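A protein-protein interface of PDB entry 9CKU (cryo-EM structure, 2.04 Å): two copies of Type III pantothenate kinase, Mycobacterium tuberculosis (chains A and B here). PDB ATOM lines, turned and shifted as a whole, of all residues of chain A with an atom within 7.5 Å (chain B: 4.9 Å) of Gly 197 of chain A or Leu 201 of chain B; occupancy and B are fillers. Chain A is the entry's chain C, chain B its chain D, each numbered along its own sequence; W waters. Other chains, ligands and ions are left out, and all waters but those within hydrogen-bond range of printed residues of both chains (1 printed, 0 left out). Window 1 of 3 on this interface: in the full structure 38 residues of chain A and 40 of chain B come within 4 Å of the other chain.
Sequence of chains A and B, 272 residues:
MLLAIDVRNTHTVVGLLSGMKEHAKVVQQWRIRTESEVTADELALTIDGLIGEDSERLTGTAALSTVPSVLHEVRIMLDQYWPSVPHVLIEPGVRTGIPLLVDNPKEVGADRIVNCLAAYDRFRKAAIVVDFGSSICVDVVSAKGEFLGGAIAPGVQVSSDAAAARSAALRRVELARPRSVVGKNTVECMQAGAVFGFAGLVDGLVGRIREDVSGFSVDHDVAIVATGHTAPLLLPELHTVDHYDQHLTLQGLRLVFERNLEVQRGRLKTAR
The backbone carbonyl oxygen of Gly 200 of chain A lies close to the backbone carbonyl oxygen of Gly 200 of chain B (3.3 Å).
CD2 of Leu 205 of chain B touches CB of Phe 196 of chain A, at 3.7 Å.
Leu 201 of chain B touches Gly 197 of chain A (CA to O, 3.4 Å).
CD2 of Leu 205 of chain B touches N of Gly 197 of chain A, 3.7 Å away.
Leu 201 of chain B touches Gly 200 of chain A (N to C, 3.8 Å).
Gly 197 of chain B touches Leu 201 of chain A.
Phe 198 of chain B touches Leu 201 of chain A.
Leu 201 of chain A touches Gly 200 of chain B.
Leu 201 of chain A touches Leu 201 of chain B (N to N, 3.7 Å).
Leu 205 of chain A touches Gly 197 of chain B.
Gly 197 of chain A touches Leu 201 of chain B, and with the chains exchanged Leu 201 of chain A touches Gly 197 of chain B.
Gly 197 of chain A touches Leu 205 of chain B, and with the chains exchanged Leu 205 of chain A touches Gly 197 of chain B.
Leu 201 of chain A touches Phe 198 of chain B, but with the chains exchanged Phe 198 of chain A does not touch Leu 201 of chain B (4.1 Å).
Leu 201 of chain B touches its own counterpart, Leu 201 of chain A.
9 positions are printed for both chains.
Hydrophobic or aromatic side chains of chain B within 4 Å of the printed part of chain A: Leu 201 and Leu 205.
Of the 18 printed residues of chain A, 5 touch a printed residue of chain B.
Hydrophobic or aromatic side chains of chain A within 4 Å of the printed part of chain B: Phe 196, Leu 201 and Leu 205.
Among the printed residues, 10 pairs touch across the chains.
Water W1 bridges the backbone carbonyl oxygen of Gly 200 of chain A (2.7 Å) and the backbone carbonyl oxygen of Gly 200 of chain B (2.7 Å).
Gly 197 of chain A touches just these residues of chain B: Leu 201 (3.4 Å) and Leu 205 (3.7 Å).
Of the printed residues of chain A, Leu 201 of chain B touches Gly 197, Gly 200 and Leu 201.
Of chain A, only Gly 200 (3.3 Å) and Leu 201 (3.8 Å) come within 4 Å of Gly 200 of chain B.
Of the printed residues of chain B, Phe 196 of chain A touches Leu 205.
Of the printed residues of chain A, Phe 198 of chain B touches Leu 201.
Gln 157 of chain A touches none of the printed residues of chain B.
Gln 191 of chain A touches none of the printed residues of chain B.
The nearest residue of chain A that does not touch Leu 201 of chain B is Phe 198 of chain A (4.1 Å).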
ATOM      1  N   GLN A 157      32.507 -14.746  -7.127  1.00  0.00           N
ATOM      2  CA  GLN A 157      32.799 -14.797  -5.700  1.00  0.00           C
ATOM      3  C   GLN A 157      32.043 -13.712  -4.942  1.00  0.00           C
ATOM      4  O   GLN A 157      31.683 -12.678  -5.505  1.00  0.00           O
ATOM      5  CB  GLN A 157      34.300 -14.568  -5.482  1.00  0.00           C
ATOM      6  CG  GLN A 157      34.721 -13.174  -5.998  1.00  0.00           C
ATOM      7  CD  GLN A 157      36.218 -12.962  -6.094  1.00  0.00           C
ATOM      8  OE1 GLN A 157      36.881 -12.695  -5.096  1.00  0.00           O
ATOM      9  NE2 GLN A 157      36.750 -13.048  -7.305  1.00  0.00           N
ATOM     10  N   VAL A 181      17.008 -10.188  -5.515  1.00  0.00           N
ATOM     11  CA  VAL A 181      18.131  -9.287  -5.745  1.00  0.00           C
ATOM     12  C   VAL A 181      18.288  -8.313  -4.580  1.00  0.00           C
ATOM     13  O   VAL A 181      19.408  -7.966  -4.196  1.00  0.00           O
ATOM     14  CB  VAL A 181      17.960  -8.558  -7.092  1.00  0.00           C
ATOM     15  CG1 VAL A 181      16.788  -7.591  -7.051  1.00  0.00           C
ATOM     16  CG2 VAL A 181      19.233  -7.838  -7.467  1.00  0.00           C
ATOM     17  N   GLN A 191      25.033 -12.767  -1.401  1.00  0.00           N
ATOM     18  CA  GLN A 191      24.685 -13.730  -2.438  1.00  0.00           C
ATOM     19  C   GLN A 191      24.099 -13.047  -3.666  1.00  0.00           C
ATOM     20  O   GLN A 191      24.409 -13.430  -4.798  1.00  0.00           O
ATOM     21  CB  GLN A 191      23.720 -14.767  -1.876  1.00  0.00           C
ATOM     22  CG  GLN A 191      24.390 -15.692  -0.888  1.00  0.00           C
ATOM     23  CD  GLN A 191      23.434 -16.669  -0.250  1.00  0.00           C
ATOM     24  OE1 GLN A 191      22.221 -16.507  -0.324  1.00  0.00           O
ATOM     25  NE2 GLN A 191      23.981 -17.696   0.384  1.00  0.00           N
ATOM     26  N   ALA A 192      23.231 -12.055  -3.468  1.00  0.00           N
ATOM     27  CA  ALA A 192      22.690 -11.318  -4.599  1.00  0.00           C
ATOM     28  C   ALA A 192      23.813 -10.640  -5.363  1.00  0.00           C
ATOM     29  O   ALA A 192      23.913 -10.774  -6.585  1.00  0.00           O
ATOM     30  CB  ALA A 192      21.657 -10.295  -4.125  1.00  0.00           C
ATOM     31  N   GLY A 193      24.706  -9.966  -4.644  1.00  0.00           N
ATOM     32  CA  GLY A 193      25.876  -9.384  -5.256  1.00  0.00           C
ATOM     33  C   GLY A 193      26.601 -10.401  -6.104  1.00  0.00           C
ATOM     34  O   GLY A 193      26.615 -10.264  -7.317  1.00  0.00           O
ATOM     35  N   ALA A 194      27.081 -11.489  -5.509  1.00  0.00           N
ATOM     36  CA  ALA A 194      27.833 -12.476  -6.276  1.00  0.00           C
ATOM     37  C   ALA A 194      27.050 -12.948  -7.500  1.00  0.00           C
ATOM     38  O   ALA A 194      27.437 -12.681  -8.641  1.00  0.00           O
ATOM     39  CB  ALA A 194      28.197 -13.656  -5.378  1.00  0.00           C
ATOM     40  N   VAL A 195      25.905 -13.589  -7.279  1.00  0.00           N
ATOM     41  CA  VAL A 195      25.233 -14.298  -8.362  1.00  0.00           C
ATOM     42  C   VAL A 195      24.746 -13.317  -9.423  1.00  0.00           C
ATOM     43  O   VAL A 195      25.139 -13.405 -10.596  1.00  0.00           O
ATOM     44  CB  VAL A 195      24.091 -15.171  -7.805  1.00  0.00           C
ATOM     45  CG1 VAL A 195      23.298 -15.830  -8.925  1.00  0.00           C
ATOM     46  CG2 VAL A 195      24.661 -16.236  -6.874  1.00  0.00           C
ATOM     47  N   PHE A 196      23.877 -12.372  -9.038  1.00  0.00           N
ATOM     48  CA  PHE A 196      23.302 -11.483 -10.035  1.00  0.00           C
ATOM     49  C   PHE A 196      24.351 -10.537 -10.619  1.00  0.00           C
ATOM     50  O   PHE A 196      24.323 -10.259 -11.819  1.00  0.00           O
ATOM     51  CB  PHE A 196      22.126 -10.709  -9.432  1.00  0.00           C
ATOM     52  CG  PHE A 196      20.981 -11.584  -8.988  1.00  0.00           C
ATOM     53  CD1 PHE A 196      20.322 -12.411  -9.888  1.00  0.00           C
ATOM     54  CD2 PHE A 196      20.561 -11.580  -7.671  1.00  0.00           C
ATOM     55  CE1 PHE A 196      19.269 -13.211  -9.482  1.00  0.00           C
ATOM     56  CE2 PHE A 196      19.509 -12.380  -7.259  1.00  0.00           C
ATOM     57  CZ  PHE A 196      18.865 -13.198  -8.165  1.00  0.00           C
ATOM     58  N   GLY A 197      25.285 -10.016  -9.811  1.00  0.00           N
ATOM     59  CA  GLY A 197      26.299  -9.139 -10.347  1.00  0.00           C
ATOM     60  C   GLY A 197      27.207  -9.819 -11.351  1.00  0.00           C
ATOM     61  O   GLY A 197      27.543  -9.232 -12.371  1.00  0.00           O
ATOM     62  N   PHE A 198      27.631 -11.061 -11.083  1.00  0.00           N
ATOM     63  CA  PHE A 198      28.510 -11.705 -12.052  1.00  0.00           C
ATOM     64  C   PHE A 198      27.747 -12.177 -13.283  1.00  0.00           C
ATOM     65  O   PHE A 198      28.316 -12.195 -14.380  1.00  0.00           O
ATOM     66  CB  PHE A 198      29.291 -12.842 -11.397  1.00  0.00           C
ATOM     67  CG  PHE A 198      30.537 -12.374 -10.708  1.00  0.00           C
ATOM     68  CD1 PHE A 198      31.707 -12.180 -11.421  1.00  0.00           C
ATOM     69  CD2 PHE A 198      30.537 -12.105  -9.351  1.00  0.00           C
ATOM     70  CE1 PHE A 198      32.851 -11.738 -10.796  1.00  0.00           C
ATOM     71  CE2 PHE A 198      31.675 -11.660  -8.721  1.00  0.00           C
ATOM     72  CZ  PHE A 198      32.839 -11.479  -9.447  1.00  0.00           C
ATOM     73  N   ALA A 199      26.460 -12.508 -13.147  1.00  0.00           N
ATOM     74  CA  ALA A 199      25.646 -12.672 -14.345  1.00  0.00           C
ATOM     75  C   ALA A 199      25.635 -11.384 -15.163  1.00  0.00           C
ATOM     76  O   ALA A 199      25.804 -11.416 -16.387  1.00  0.00           O
ATOM     77  CB  ALA A 199      24.226 -13.087 -13.969  1.00  0.00           C
ATOM     78  N   GLY A 200      25.457 -10.239 -14.499  1.00  0.00           N
ATOM     79  CA  GLY A 200      25.502  -8.967 -15.200  1.00  0.00           C
ATOM     80  C   GLY A 200      26.860  -8.685 -15.815  1.00  0.00           C
ATOM     81  O   GLY A 200      26.948  -8.131 -16.904  1.00  0.00           O
ATOM     82  N   LEU A 201      27.931  -9.076 -15.129  1.00  0.00           N
ATOM     83  CA  LEU A 201      29.280  -8.878 -15.653  1.00  0.00           C
ATOM     84  C   LEU A 201      29.487  -9.661 -16.946  1.00  0.00           C
ATOM     85  O   LEU A 201      29.978  -9.119 -17.946  1.00  0.00           O
ATOM     86  CB  LEU A 201      30.311  -9.288 -14.600  1.00  0.00           C
ATOM     87  CG  LEU A 201      31.783  -9.246 -15.026  1.00  0.00           C
ATOM     88  CD1 LEU A 201      32.653  -8.733 -13.887  1.00  0.00           C
ATOM     89  CD2 LEU A 201      32.292 -10.601 -15.519  1.00  0.00           C
ATOM     90  N   VAL A 202      29.106 -10.940 -16.945  1.00  0.00           N
ATOM     91  CA  VAL A 202      29.251 -11.756 -18.150  1.00  0.00           C
ATOM     92  C   VAL A 202      28.377 -11.205 -19.271  1.00  0.00           C
ATOM     93  O   VAL A 202      28.817 -11.086 -20.422  1.00  0.00           O
ATOM     94  CB  VAL A 202      28.928 -13.234 -17.855  1.00  0.00           C
ATOM     95  CG1 VAL A 202      28.734 -14.014 -19.153  1.00  0.00           C
ATOM     96  CG2 VAL A 202      30.034 -13.872 -17.017  1.00  0.00           C
ATOM     97  N   ASP A 203      27.114 -10.896 -18.961  1.00  0.00           N
ATOM     98  CA  ASP A 203      26.228 -10.350 -19.979  1.00  0.00           C
ATOM     99  C   ASP A 203      26.777  -9.047 -20.538  1.00  0.00           C
ATOM    100  O   ASP A 203      26.732  -8.826 -21.748  1.00  0.00           O
ATOM    101  CB  ASP A 203      24.822 -10.141 -19.414  1.00  0.00           C
ATOM    102  CG  ASP A 203      24.005 -11.422 -19.375  1.00  0.00           C
ATOM    103  OD1 ASP A 203      24.349 -12.387 -20.086  1.00  0.00           O
ATOM    104  OD2 ASP A 203      23.002 -11.460 -18.636  1.00  0.00           O
ATOM    105  N   GLY A 204      27.319  -8.183 -19.681  1.00  0.00           N
ATOM    106  CA  GLY A 204      27.887  -6.940 -20.162  1.00  0.00           C
ATOM    107  C   GLY A 204      29.058  -7.161 -21.093  1.00  0.00           C
ATOM    108  O   GLY A 204      29.143  -6.536 -22.147  1.00  0.00           O
ATOM    109  N   LEU A 205      29.964  -8.066 -20.730  1.00  0.00           N
ATOM    110  CA  LEU A 205      31.113  -8.328 -21.593  1.00  0.00           C
ATOM    111  C   LEU A 205      30.671  -8.887 -22.942  1.00  0.00           C
ATOM    112  O   LEU A 205      31.125  -8.425 -23.995  1.00  0.00           O
ATOM    113  CB  LEU A 205      32.088  -9.279 -20.900  1.00  0.00           C
ATOM    114  CG  LEU A 205      32.918  -8.676 -19.762  1.00  0.00           C
ATOM    115  CD1 LEU A 205      33.764  -9.734 -19.092  1.00  0.00           C
ATOM    116  CD2 LEU A 205      33.796  -7.535 -20.257  1.00  0.00           C
ATOM    117  N   LEU A 234      25.301 -19.788 -12.553  1.00  0.00           N
ATOM    118  CA  LEU A 234      24.981 -18.533 -13.216  1.00  0.00           C
ATOM    119  C   LEU A 234      24.151 -18.694 -14.479  1.00  0.00           C
ATOM    120  O   LEU A 234      23.523 -17.723 -14.904  1.00  0.00           O
ATOM    121  CB  LEU A 234      26.267 -17.784 -13.576  1.00  0.00           C
ATOM    122  CG  LEU A 234      26.704 -16.690 -12.602  1.00  0.00           C
ATOM    123  CD1 LEU A 234      27.142 -17.284 -11.280  1.00  0.00           C
ATOM    124  CD2 LEU A 234      27.811 -15.845 -13.210  1.00  0.00           C
ATOM    125  N   ILE B 136      31.190  -3.048  -3.880  1.00  0.00           N
ATOM    126  CA  ILE B 136      30.157  -2.274  -4.557  1.00  0.00           C
ATOM    127  C   ILE B 136      28.846  -2.555  -3.834  1.00  0.00           C
ATOM    128  O   ILE B 136      28.357  -3.685  -3.830  1.00  0.00           O
ATOM    129  CB  ILE B 136      30.066  -2.614  -6.048  1.00  0.00           C
ATOM    130  CG1 ILE B 136      31.344  -2.165  -6.758  1.00  0.00           C
ATOM    131  CG2 ILE B 136      28.842  -1.937  -6.668  1.00  0.00           C
ATOM    132  CD1 ILE B 136      31.440  -2.602  -8.194  1.00  0.00           C
ATOM    133  N   ALA B 153      28.509  -6.558  -3.677  1.00  0.00           N
ATOM    134  CA  ALA B 153      29.337  -7.250  -4.646  1.00  0.00           C
ATOM    135  C   ALA B 153      30.805  -6.927  -4.408  1.00  0.00           C
ATOM    136  O   ALA B 153      31.129  -5.933  -3.752  1.00  0.00           O
ATOM    137  CB  ALA B 153      28.949  -6.847  -6.077  1.00  0.00           C
ATOM    138  N   GLY B 197      33.558  -5.337 -17.353  1.00  0.00           N
ATOM    139  CA  GLY B 197      32.791  -6.305 -16.606  1.00  0.00           C
ATOM    140  C   GLY B 197      32.140  -5.732 -15.365  1.00  0.00           C
ATOM    141  O   GLY B 197      31.015  -6.092 -15.041  1.00  0.00           O
ATOM    142  N   PHE B 198      32.829  -4.846 -14.637  1.00  0.00           N
ATOM    143  CA  PHE B 198      32.175  -4.280 -13.466  1.00  0.00           C
ATOM    144  C   PHE B 198      31.145  -3.229 -13.855  1.00  0.00           C
ATOM    145  O   PHE B 198      30.145  -3.069 -13.148  1.00  0.00           O
ATOM    146  CB  PHE B 198      33.211  -3.725 -12.493  1.00  0.00           C
ATOM    147  CG  PHE B 198      33.783  -4.773 -11.587  1.00  0.00           C
ATOM    148  CD1 PHE B 198      33.135  -5.124 -10.417  1.00  0.00           C
ATOM    149  CD2 PHE B 198      34.958  -5.426 -11.916  1.00  0.00           C
ATOM    150  CE1 PHE B 198      33.653  -6.097  -9.591  1.00  0.00           C
ATOM    151  CE2 PHE B 198      35.480  -6.397 -11.092  1.00  0.00           C
ATOM    152  CZ  PHE B 198      34.827  -6.732  -9.929  1.00  0.00           C
ATOM    153  N   ALA B 199      31.328  -2.547 -14.990  1.00  0.00           N
ATOM    154  CA  ALA B 199      30.224  -1.757 -15.523  1.00  0.00           C
ATOM    155  C   ALA B 199      29.012  -2.643 -15.789  1.00  0.00           C
ATOM    156  O   ALA B 199      27.882  -2.288 -15.440  1.00  0.00           O
ATOM    157  CB  ALA B 199      30.654  -1.035 -16.798  1.00  0.00           C
ATOM    158  N   GLY B 200      29.241  -3.819 -16.378  1.00  0.00           N
ATOM    159  CA  GLY B 200      28.152  -4.760 -16.591  1.00  0.00           C
ATOM    160  C   GLY B 200      27.550  -5.268 -15.294  1.00  0.00           C
ATOM    161  O   GLY B 200      26.341  -5.434 -15.188  1.00  0.00           O
ATOM    162  N   LEU B 201      28.389  -5.521 -14.293  1.00  0.00           N
ATOM    163  CA  LEU B 201      27.896  -5.953 -12.988  1.00  0.00           C
ATOM    164  C   LEU B 201      26.936  -4.924 -12.396  1.00  0.00           C
ATOM    165  O   LEU B 201      25.823  -5.260 -11.967  1.00  0.00           O
ATOM    166  CB  LEU B 201      29.069  -6.187 -12.036  1.00  0.00           C
ATOM    167  CG  LEU B 201      28.694  -6.606 -10.609  1.00  0.00           C
ATOM    168  CD1 LEU B 201      29.661  -7.656 -10.088  1.00  0.00           C
ATOM    169  CD2 LEU B 201      28.636  -5.428  -9.637  1.00  0.00           C
ATOM    170  N   VAL B 202      27.356  -3.659 -12.359  1.00  0.00           N
ATOM    171  CA  VAL B 202      26.506  -2.613 -11.795  1.00  0.00           C
ATOM    172  C   VAL B 202      25.229  -2.475 -12.613  1.00  0.00           C
ATOM    173  O   VAL B 202      24.126  -2.363 -12.062  1.00  0.00           O
ATOM    174  CB  VAL B 202      27.264  -1.274 -11.717  1.00  0.00           C
ATOM    175  CG1 VAL B 202      26.306  -0.144 -11.364  1.00  0.00           C
ATOM    176  CG2 VAL B 202      28.393  -1.350 -10.698  1.00  0.00           C
ATOM    177  N   ASP B 203      25.361  -2.435 -13.940  1.00  0.00           N
ATOM    178  CA  ASP B 203      24.183  -2.272 -14.779  1.00  0.00           C
ATOM    179  C   ASP B 203      23.218  -3.428 -14.590  1.00  0.00           C
ATOM    180  O   ASP B 203      22.006  -3.220 -14.532  1.00  0.00           O
ATOM    181  CB  ASP B 203      24.588  -2.132 -16.245  1.00  0.00           C
ATOM    182  CG  ASP B 203      25.031  -0.718 -16.600  1.00  0.00           C
ATOM    183  OD1 ASP B 203      24.943   0.184 -15.741  1.00  0.00           O
ATOM    184  OD2 ASP B 203      25.466  -0.505 -17.748  1.00  0.00           O
ATOM    185  N   GLY B 204      23.739  -4.649 -14.460  1.00  0.00           N
ATOM    186  CA  GLY B 204      22.883  -5.793 -14.241  1.00  0.00           C
ATOM    187  C   GLY B 204      22.156  -5.730 -12.916  1.00  0.00           C
ATOM    188  O   GLY B 204      20.962  -6.009 -12.849  1.00  0.00           O
ATOM    189  N   LEU B 205      22.856  -5.347 -11.848  1.00  0.00           N
ATOM    190  CA  LEU B 205      22.188  -5.242 -10.553  1.00  0.00           C
ATOM    191  C   LEU B 205      21.088  -4.184 -10.588  1.00  0.00           C
ATOM    192  O   LEU B 205      19.970  -4.420 -10.116  1.00  0.00           O
ATOM    193  CB  LEU B 205      23.203  -4.937  -9.452  1.00  0.00           C
ATOM    194  CG  LEU B 205      24.088  -6.102  -9.002  1.00  0.00           C
ATOM    195  CD1 LEU B 205      25.073  -5.642  -7.950  1.00  0.00           C
ATOM    196  CD2 LEU B 205      23.252  -7.263  -8.486  1.00  0.00           C
HETATM  197  O   HOH W   1      25.146  -6.189 -17.517  1.00  0.00           O
